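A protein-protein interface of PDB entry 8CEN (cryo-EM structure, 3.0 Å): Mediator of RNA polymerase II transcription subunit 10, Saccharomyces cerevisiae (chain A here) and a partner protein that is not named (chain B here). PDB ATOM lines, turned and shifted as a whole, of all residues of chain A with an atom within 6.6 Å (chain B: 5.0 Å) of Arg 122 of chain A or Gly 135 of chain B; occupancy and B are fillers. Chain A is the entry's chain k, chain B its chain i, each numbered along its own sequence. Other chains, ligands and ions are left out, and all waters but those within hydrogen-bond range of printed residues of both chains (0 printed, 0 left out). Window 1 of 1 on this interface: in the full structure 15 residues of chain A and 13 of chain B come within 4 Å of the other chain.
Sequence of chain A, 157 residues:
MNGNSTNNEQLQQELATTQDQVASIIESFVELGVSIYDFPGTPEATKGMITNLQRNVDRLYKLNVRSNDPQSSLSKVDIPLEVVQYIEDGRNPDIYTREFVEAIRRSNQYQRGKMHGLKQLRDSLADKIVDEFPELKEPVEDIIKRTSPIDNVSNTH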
ATOM      1  N   GLY A 117      -0.296 -16.696  -9.023  1.00  0.00           N
ATOM      2  CA  GLY A 117      -0.830 -16.017  -7.854  1.00  0.00           C
ATOM      3  C   GLY A 117      -1.260 -14.596  -8.163  1.00  0.00           C
ATOM      4  O   GLY A 117      -2.298 -14.130  -7.681  1.00  0.00           O
ATOM      5  N   LEU A 118      -0.480 -13.896  -8.988  1.00  0.00           N
ATOM      6  CA  LEU A 118      -0.855 -12.552  -9.401  1.00  0.00           C
ATOM      7  C   LEU A 118      -2.096 -12.566 -10.286  1.00  0.00           C
ATOM      8  O   LEU A 118      -2.913 -11.646 -10.212  1.00  0.00           O
ATOM      9  CB  LEU A 118       0.323 -11.896 -10.116  1.00  0.00           C
ATOM     10  CG  LEU A 118       1.364 -11.270  -9.188  1.00  0.00           C
ATOM     11  CD1 LEU A 118       2.609 -10.894  -9.963  1.00  0.00           C
ATOM     12  CD2 LEU A 118       0.786 -10.059  -8.478  1.00  0.00           C
ATOM     13  N   LYS A 119      -2.273 -13.612 -11.098  1.00  0.00           N
ATOM     14  CA  LYS A 119      -3.485 -13.735 -11.905  1.00  0.00           C
ATOM     15  C   LYS A 119      -4.707 -14.020 -11.034  1.00  0.00           C
ATOM     16  O   LYS A 119      -5.803 -13.511 -11.307  1.00  0.00           O
ATOM     17  CB  LYS A 119      -3.298 -14.831 -12.955  1.00  0.00           C
ATOM     18  CG  LYS A 119      -4.422 -14.944 -13.970  1.00  0.00           C
ATOM     19  CD  LYS A 119      -4.101 -16.011 -15.005  1.00  0.00           C
ATOM     20  CE  LYS A 119      -5.216 -16.163 -16.027  1.00  0.00           C
ATOM     21  NZ  LYS A 119      -4.906 -17.224 -17.025  1.00  0.00           N
ATOM     22  N   GLN A 120      -4.537 -14.840  -9.991  1.00  0.00           N
ATOM     23  CA  GLN A 120      -5.620 -15.078  -9.038  1.00  0.00           C
ATOM     24  C   GLN A 120      -6.003 -13.797  -8.307  1.00  0.00           C
ATOM     25  O   GLN A 120      -7.194 -13.492  -8.147  1.00  0.00           O
ATOM     26  CB  GLN A 120      -5.208 -16.155  -8.034  1.00  0.00           C
ATOM     27  CG  GLN A 120      -5.490 -17.576  -8.481  1.00  0.00           C
ATOM     28  CD  GLN A 120      -4.539 -18.575  -7.853  1.00  0.00           C
ATOM     29  OE1 GLN A 120      -3.846 -18.264  -6.885  1.00  0.00           O
ATOM     30  NE2 GLN A 120      -4.506 -19.785  -8.398  1.00  0.00           N
ATOM     31  N   LEU A 121      -5.002 -13.026  -7.873  1.00  0.00           N
ATOM     32  CA  LEU A 121      -5.272 -11.732  -7.258  1.00  0.00           C
ATOM     33  C   LEU A 121      -5.978 -10.798  -8.232  1.00  0.00           C
ATOM     34  O   LEU A 121      -6.951 -10.126  -7.864  1.00  0.00           O
ATOM     35  CB  LEU A 121      -3.969 -11.106  -6.764  1.00  0.00           C
ATOM     36  CG  LEU A 121      -4.068  -9.681  -6.219  1.00  0.00           C
ATOM     37  CD1 LEU A 121      -5.007  -9.635  -5.024  1.00  0.00           C
ATOM     38  CD2 LEU A 121      -2.693  -9.145  -5.855  1.00  0.00           C
ATOM     39  N   ARG A 122      -5.531 -10.789  -9.491  1.00  0.00           N
ATOM     40  CA  ARG A 122      -6.089  -9.895 -10.499  1.00  0.00           C
ATOM     41  C   ARG A 122      -7.554 -10.200 -10.770  1.00  0.00           C
ATOM     42  O   ARG A 122      -8.401  -9.303 -10.706  1.00  0.00           O
ATOM     43  CB  ARG A 122      -5.278  -9.996 -11.791  1.00  0.00           C
ATOM     44  CG  ARG A 122      -5.849  -9.185 -12.940  1.00  0.00           C
ATOM     45  CD  ARG A 122      -5.396  -9.733 -14.282  1.00  0.00           C
ATOM     46  NE  ARG A 122      -6.274 -10.791 -14.765  1.00  0.00           N
ATOM     47  CZ  ARG A 122      -6.228 -11.303 -15.986  1.00  0.00           C
ATOM     48  NH1 ARG A 122      -5.356 -10.874 -16.883  1.00  0.00           N
ATOM     49  NH2 ARG A 122      -7.080 -12.269 -16.318  1.00  0.00           N
ATOM     50  N   ASP A 123      -7.886 -11.462 -11.057  1.00  0.00           N
ATOM     51  CA  ASP A 123      -9.275 -11.724 -11.422  1.00  0.00           C
ATOM     52  C   ASP A 123     -10.202 -11.733 -10.208  1.00  0.00           C
ATOM     53  O   ASP A 123     -11.362 -11.323 -10.339  1.00  0.00           O
ATOM     54  CB  ASP A 123      -9.408 -13.007 -12.264  1.00  0.00           C
ATOM     55  CG  ASP A 123      -8.983 -14.272 -11.541  1.00  0.00           C
ATOM     56  OD1 ASP A 123      -8.537 -14.213 -10.390  1.00  0.00           O
ATOM     57  OD2 ASP A 123      -9.107 -15.356 -12.149  1.00  0.00           O
ATOM     58  N   SER A 124      -9.719 -12.127  -9.017  1.00  0.00           N
ATOM     59  CA  SER A 124     -10.557 -12.001  -7.826  1.00  0.00           C
ATOM     60  C   SER A 124     -10.850 -10.539  -7.501  1.00  0.00           C
ATOM     61  O   SER A 124     -12.006 -10.176  -7.231  1.00  0.00           O
ATOM     62  CB  SER A 124      -9.890 -12.691  -6.637  1.00  0.00           C
ATOM     63  OG  SER A 124      -8.581 -12.191  -6.428  1.00  0.00           O
ATOM     64  N   LEU A 125      -9.822  -9.681  -7.547  1.00  0.00           N
ATOM     65  CA  LEU A 125     -10.026  -8.264  -7.281  1.00  0.00           C
ATOM     66  C   LEU A 125     -10.891  -7.619  -8.354  1.00  0.00           C
ATOM     67  O   LEU A 125     -11.716  -6.755  -8.045  1.00  0.00           O
ATOM     68  CB  LEU A 125      -8.675  -7.555  -7.174  1.00  0.00           C
ATOM     69  CG  LEU A 125      -8.682  -6.051  -6.903  1.00  0.00           C
ATOM     70  CD1 LEU A 125      -9.500  -5.723  -5.664  1.00  0.00           C
ATOM     71  CD2 LEU A 125      -7.260  -5.544  -6.762  1.00  0.00           C
ATOM     72  N   ALA A 126     -10.732  -8.035  -9.613  1.00  0.00           N
ATOM     73  CA  ALA A 126     -11.554  -7.496 -10.694  1.00  0.00           C
ATOM     74  C   ALA A 126     -13.020  -7.868 -10.521  1.00  0.00           C
ATOM     75  O   ALA A 126     -13.905  -7.019 -10.693  1.00  0.00           O
ATOM     76  CB  ALA A 126     -11.028  -7.992 -12.039  1.00  0.00           C
ATOM     77  N   ASP A 127     -13.293  -9.130 -10.165  1.00  0.00           N
ATOM     78  CA  ASP A 127     -14.668  -9.553  -9.926  1.00  0.00           C
ATOM     79  C   ASP A 127     -15.279  -8.804  -8.749  1.00  0.00           C
ATOM     80  O   ASP A 127     -16.444  -8.394  -8.806  1.00  0.00           O
ATOM     81  CB  ASP A 127     -14.725 -11.061  -9.685  1.00  0.00           C
ATOM     82  CG  ASP A 127     -14.359 -11.861 -10.917  1.00  0.00           C
ATOM     83  OD1 ASP A 127     -14.353 -11.281 -12.023  1.00  0.00           O
ATOM     84  OD2 ASP A 127     -14.074 -13.070 -10.779  1.00  0.00           O
ATOM     85  N   ILE A 143      -9.477  -3.621 -18.886  1.00  0.00           N
ATOM     86  CA  ILE A 143      -8.205  -3.880 -18.215  1.00  0.00           C
ATOM     87  C   ILE A 143      -7.861  -5.366 -18.253  1.00  0.00           C
ATOM     88  O   ILE A 143      -6.713  -5.740 -18.521  1.00  0.00           O
ATOM     89  CB  ILE A 143      -8.253  -3.327 -16.777  1.00  0.00           C
ATOM     90  CG1 ILE A 143      -8.073  -1.809 -16.798  1.00  0.00           C
ATOM     91  CG2 ILE A 143      -7.200  -3.973 -15.888  1.00  0.00           C
ATOM     92  CD1 ILE A 143      -8.232  -1.162 -15.453  1.00  0.00           C
ATOM     93  N   ILE A 144      -8.847  -6.232 -18.006  1.00  0.00           N
ATOM     94  CA  ILE A 144      -8.614  -7.673 -18.056  1.00  0.00           C
ATOM     95  C   ILE A 144      -8.279  -8.118 -19.477  1.00  0.00           C
ATOM     96  O   ILE A 144      -7.375  -8.934 -19.683  1.00  0.00           O
ATOM     97  CB  ILE A 144      -9.822  -8.437 -17.481  1.00  0.00           C
ATOM     98  CG1 ILE A 144     -10.009  -8.107 -15.998  1.00  0.00           C
ATOM     99  CG2 ILE A 144      -9.660  -9.940 -17.652  1.00  0.00           C
ATOM    100  CD1 ILE A 144      -8.839  -8.506 -15.133  1.00  0.00           C
ATOM    101  N   LYS A 145      -8.974  -7.567 -20.479  1.00  0.00           N
ATOM    102  CA  LYS A 145      -8.674  -7.910 -21.868  1.00  0.00           C
ATOM    103  C   LYS A 145      -7.280  -7.444 -22.276  1.00  0.00           C
ATOM    104  O   LYS A 145      -6.577  -8.145 -23.012  1.00  0.00           O
ATOM    105  CB  LYS A 145      -9.731  -7.307 -22.792  1.00  0.00           C
ATOM    106  CG  LYS A 145     -10.970  -8.171 -22.967  1.00  0.00           C
ATOM    107  CD  LYS A 145     -12.036  -7.456 -23.784  1.00  0.00           C
ATOM    108  CE  LYS A 145     -11.496  -6.994 -25.127  1.00  0.00           C
ATOM    109  NZ  LYS A 145     -12.134  -5.725 -25.574  1.00  0.00           N
ATOM    110  N   ARG A 146      -6.862  -6.267 -21.806  1.00  0.00           N
ATOM    111  CA  ARG A 146      -5.554  -5.740 -22.181  1.00  0.00           C
ATOM    112  C   ARG A 146      -4.430  -6.465 -21.452  1.00  0.00           C
ATOM    113  O   ARG A 146      -3.356  -6.690 -22.024  1.00  0.00           O
ATOM    114  CB  ARG A 146      -5.509  -4.241 -21.904  1.00  0.00           C
ATOM    115  CG  ARG A 146      -6.142  -3.413 -23.009  1.00  0.00           C
ATOM    116  CD  ARG A 146      -6.367  -1.927 -22.679  1.00  0.00           C
ATOM    117  NE  ARG A 146      -5.232  -1.223 -22.090  1.00  0.00           N
ATOM    118  CZ  ARG A 146      -5.007  -1.088 -20.789  1.00  0.00           C
ATOM    119  NH1 ARG A 146      -5.841  -1.581 -19.888  1.00  0.00           N
ATOM    120  NH2 ARG A 146      -3.925  -0.431 -20.383  1.00  0.00           N
ATOM    121  N   THR A 147      -4.654  -6.842 -20.197  1.00  0.00           N
ATOM    122  CA  THR A 147      -3.670  -7.579 -19.419  1.00  0.00           C
ATOM    123  C   THR A 147      -3.787  -9.084 -19.603  1.00  0.00           C
ATOM    124  O   THR A 147      -3.082  -9.831 -18.925  1.00  0.00           O
ATOM    125  CB  THR A 147      -3.794  -7.229 -17.933  1.00  0.00           C
ATOM    126  OG1 THR A 147      -5.123  -7.513 -17.479  1.00  0.00           O
ATOM    127  CG2 THR A 147      -3.481  -5.756 -17.703  1.00  0.00           C
ATOM    128  N   SER A 148      -4.690  -9.544 -20.463  1.00  0.00           N
ATOM    129  CA  SER A 148      -4.693 -10.920 -20.958  1.00  0.00           C
ATOM    130  C   SER A 148      -4.752 -10.871 -22.480  1.00  0.00           C
ATOM    131  O   SER A 148      -5.794 -11.146 -23.086  1.00  0.00           O
ATOM    132  CB  SER A 148      -5.865 -11.714 -20.381  1.00  0.00           C
ATOM    133  OG  SER A 148      -5.698 -13.104 -20.604  1.00  0.00           O
ATOM    134  N   PRO A 149      -3.636 -10.521 -23.135  1.00  0.00           N
ATOM    135  CA  PRO A 149      -3.663 -10.324 -24.590  1.00  0.00           C
ATOM    136  C   PRO A 149      -3.676 -11.628 -25.370  1.00  0.00           C
ATOM    137  O   PRO A 149      -3.828 -12.709 -24.792  1.00  0.00           O
ATOM    138  CB  PRO A 149      -2.376  -9.535 -24.855  1.00  0.00           C
ATOM    139  CG  PRO A 149      -1.450 -10.001 -23.791  1.00  0.00           C
ATOM    140  CD  PRO A 149      -2.292 -10.288 -22.576  1.00  0.00           C
ATOM    141  N   LEU B 131      -5.496  -2.429 -10.338  1.00  0.00           N
ATOM    142  CA  LEU B 131      -5.876  -3.669 -11.015  1.00  0.00           C
ATOM    143  C   LEU B 131      -5.050  -3.884 -12.282  1.00  0.00           C
ATOM    144  O   LEU B 131      -4.595  -5.004 -12.563  1.00  0.00           O
ATOM    145  CB  LEU B 131      -7.368  -3.643 -11.342  1.00  0.00           C
ATOM    146  CG  LEU B 131      -7.932  -4.835 -12.111  1.00  0.00           C
ATOM    147  CD1 LEU B 131      -7.755  -6.112 -11.313  1.00  0.00           C
ATOM    148  CD2 LEU B 131      -9.394  -4.608 -12.451  1.00  0.00           C
ATOM    149  N   GLU B 132      -4.823  -2.811 -13.042  1.00  0.00           N
ATOM    150  CA  GLU B 132      -3.982  -2.895 -14.230  1.00  0.00           C
ATOM    151  C   GLU B 132      -2.531  -3.193 -13.875  1.00  0.00           C
ATOM    152  O   GLU B 132      -1.855  -3.917 -14.613  1.00  0.00           O
ATOM    153  CB  GLU B 132      -4.089  -1.598 -15.028  1.00  0.00           C
ATOM    154  CG  GLU B 132      -3.537  -1.677 -16.435  1.00  0.00           C
ATOM    155  CD  GLU B 132      -3.764  -0.398 -17.208  1.00  0.00           C
ATOM    156  OE1 GLU B 132      -4.880   0.156 -17.125  1.00  0.00           O
ATOM    157  OE2 GLU B 132      -2.828   0.057 -17.899  1.00  0.00           O
ATOM    158  N   LEU B 133      -2.039  -2.654 -12.755  1.00  0.00           N
ATOM    159  CA  LEU B 133      -0.687  -2.969 -12.303  1.00  0.00           C
ATOM    160  C   LEU B 133      -0.556  -4.444 -11.946  1.00  0.00           C
ATOM    161  O   LEU B 133       0.458  -5.076 -12.262  1.00  0.00           O
ATOM    162  CB  LEU B 133      -0.311  -2.093 -11.107  1.00  0.00           C
ATOM    163  CG  LEU B 133       0.941  -2.497 -10.322  1.00  0.00           C
ATOM    164  CD1 LEU B 133       2.200  -2.251 -11.140  1.00  0.00           C
ATOM    165  CD2 LEU B 133       1.014  -1.770  -8.991  1.00  0.00           C
ATOM    166  N   ILE B 134      -1.576  -5.007 -11.292  1.00  0.00           N
ATOM    167  CA  ILE B 134      -1.563  -6.437 -10.981  1.00  0.00           C
ATOM    168  C   ILE B 134      -1.586  -7.269 -12.259  1.00  0.00           C
ATOM    169  O   ILE B 134      -0.897  -8.290 -12.360  1.00  0.00           O
ATOM    170  CB  ILE B 134      -2.724  -6.801 -10.035  1.00  0.00           C
ATOM    171  CG1 ILE B 134      -2.610  -6.016  -8.732  1.00  0.00           C
ATOM    172  CG2 ILE B 134      -2.719  -8.284  -9.711  1.00  0.00           C
ATOM    173  CD1 ILE B 134      -1.318  -6.269  -7.992  1.00  0.00           C
ATOM    174  N   GLY B 135      -2.355  -6.836 -13.263  1.00  0.00           N
ATOM    175  CA  GLY B 135      -2.350  -7.547 -14.539  1.00  0.00           C
ATOM    176  C   GLY B 135      -1.002  -7.507 -15.245  1.00  0.00           C
ATOM    177  O   GLY B 135      -0.522  -8.529 -15.762  1.00  0.00           O
ATOM    178  N   VAL B 136      -0.372  -6.328 -15.270  1.00  0.00           N
ATOM    179  CA  VAL B 136       0.949  -6.189 -15.879  1.00  0.00           C
ATOM    180  C   VAL B 136       1.981  -7.011 -15.116  1.00  0.00           C
ATOM    181  O   VAL B 136       2.856  -7.636 -15.717  1.00  0.00           O
ATOM    182  CB  VAL B 136       1.343  -4.701 -15.975  1.00  0.00           C
ATOM    183  CG1 VAL B 136       2.760  -4.540 -16.503  1.00  0.00           C
ATOM    184  CG2 VAL B 136       0.394  -3.975 -16.905  1.00  0.00           C
ATOM    185  N   LEU B 137       1.884  -7.053 -13.786  1.00  0.00           N
ATOM    186  CA  LEU B 137       2.796  -7.903 -13.028  1.00  0.00           C
ATOM    187  C   LEU B 137       2.508  -9.383 -13.253  1.00  0.00           C
ATOM    188  O   LEU B 137       3.420 -10.212 -13.149  1.00  0.00           O
ATOM    189  CB  LEU B 137       2.721  -7.572 -11.538  1.00  0.00           C
ATOM    190  CG  LEU B 137       3.313  -6.245 -11.066  1.00  0.00           C
ATOM    191  CD1 LEU B 137       2.883  -5.951  -9.639  1.00  0.00           C
ATOM    192  CD2 LEU B 137       4.823  -6.274 -11.177  1.00  0.00           C
ATOM    193  N   SER B 138       1.261  -9.733 -13.567  1.00  0.00           N
ATOM    194  CA  SER B 138       0.900 -11.127 -13.781  1.00  0.00           C
ATOM    195  C   SER B 138       1.271 -11.642 -15.163  1.00  0.00           C
ATOM    196  O   SER B 138       1.292 -12.861 -15.360  1.00  0.00           O
ATOM    197  CB  SER B 138      -0.603 -11.326 -13.576  1.00  0.00           C
ATOM    198  OG  SER B 138      -1.343 -10.633 -14.561  1.00  0.00           O
ATOM    199  N   ILE B 139       1.520 -10.765 -16.139  1.00  0.00           N
ATOM    200  CA  ILE B 139       1.929 -11.213 -17.466  1.00  0.00           C
ATOM    201  C   ILE B 139       3.367 -10.830 -17.810  1.00  0.00           C
ATOM    202  O   ILE B 139       4.091 -11.632 -18.410  1.00  0.00           O
ATOM    203  CB  ILE B 139       0.947 -10.746 -18.565  1.00  0.00           C
ATOM    204  CG1 ILE B 139       0.856  -9.219 -18.665  1.00  0.00           C
ATOM    205  CG2 ILE B 139      -0.397 -11.407 -18.360  1.00  0.00           C
ATOM    206  CD1 ILE B 139       0.089  -8.732 -19.871  1.00  0.00           C
ATOM    207  N   ASN B 140       3.812  -9.630 -17.444  1.00  0.00           N
ATOM    208  CA  ASN B 140       5.155  -9.165 -17.773  1.00  0.00           C
ATOM    209  C   ASN B 140       5.565  -8.041 -16.829  1.00  0.00           C
ATOM    210  O   ASN B 140       5.213  -6.879 -17.065  1.00  0.00           O
ATOM    211  CB  ASN B 140       5.216  -8.691 -19.229  1.00  0.00           C
ATOM    212  CG  ASN B 140       6.629  -8.352 -19.690  1.00  0.00           C
ATOM    213  OD1 ASN B 140       7.597  -8.502 -18.949  1.00  0.00           O
ATOM    214  ND2 ASN B 140       6.751  -7.939 -20.945  1.00  0.00           N
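The side-chain hydroxyl (OG) of Ser 138 of chain B lies within hydrogen-bond range of the backbone carbonyl oxygen (O) of Ile 134 of chain B (3.2 Å). The backbone carbonyl oxygen of Gly 135 of chain B is in hydrogen-bond range of the side-chain hydroxyl of Ser 138 of chain B (2.6 Å). The side-chain hydroxyl (OG) of Ser 124 of chain A is in hydrogen-bond range of the backbone carbonyl oxygen (O) of Leu 121 of chain A (3.0 Å). The guanidinium group (NH1) of Arg 122 of chain A lies within hydrogen-bond range of the backbone carbonyl oxygen (O) of Thr 147 of chain A, 3.2 Å away. The backbone carbonyl oxygen (O) of Ile 143 of chain A is in hydrogen-bond range of the side-chain hydroxyl (OG1) of Thr 147 of chain A (2.6 Å). O of Ile 144 of chain A is in hydrogen-bond range of OG1 of Thr 147 of chain A.
NH2 of Arg 146 of chain A is in salt-bridge range of OE2 of Glu 132 of chain B, at 2.8 Å.
CG2 of Ile 134 of chain B touches O of Leu 118 of chain A (3.4 Å). Leu 118 of chain A touches Leu 137 of chain B (CD1 to O, 3.4 Å). Ser 138 of chain B touches Lys 119 of chain A (CB to N, 3.8 Å). Ile 134 of chain B touches Leu 121 of chain A. Arg 122 of chain A touches Leu 131 of chain B. Arg 122 of chain A touches Ile 134 of chain B (CB to CG2, 3.7 Å). Arg 122 of chain A touches Gly 135 of chain B (CD to CA, 3.8 Å). CG of Leu 131 of chain B touches CG2 of Ile 143 of chain A, at 3.9 Å. Glu 132 of chain B touches Thr 147 of chain A. CD of Pro 149 of chain A touches CD1 of Ile 139 of chain B (3.9 Å).
Printed residues of chain A that touch a printed residue of chain B: Leu 118, Lys 119, Leu 121, Arg 122, Ala 126, Ile 143, Arg 146, Thr 147 and Pro 149. Along chain A the printed residues that touch a printed residue of chain B span positions 118 to 149. Hydrophobic or aromatic side chains of chain B within 4 Å of the printed part of chain A: Leu 131, Ile 134, Leu 137 and Ile 139. Among the printed residues, Asp or Glu carboxylates within 4 Å of a Lys or Arg side-chain nitrogen of the other chain: Arg 146 of chain A with Glu 132 of chain B (2.8 Å).
Leu 125 of chain A touches none of the printed residues of chain B. Of the printed residues of chain B, Thr 147 of chain A touches Glu 132, Gly 135, Val 136 and Ile 139. Of the printed residues of chain A, Ile 134 of chain B touches Leu 118, Leu 121 and Arg 122. Gly 135 of chain B touches just these residues of chain A: Arg 122 and Thr 147. Of the printed residues of chain A, Val 136 of chain B touches Thr 147 (3.99 Å). Of the printed residues of chain A, Ile 139 of chain B touches Thr 147 (3.2 Å) and Pro 149 (3.9 Å). The nearest residue of chain A that does not touch Gly 135 of chain B is Leu 118 of chain A (5.7 Å).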
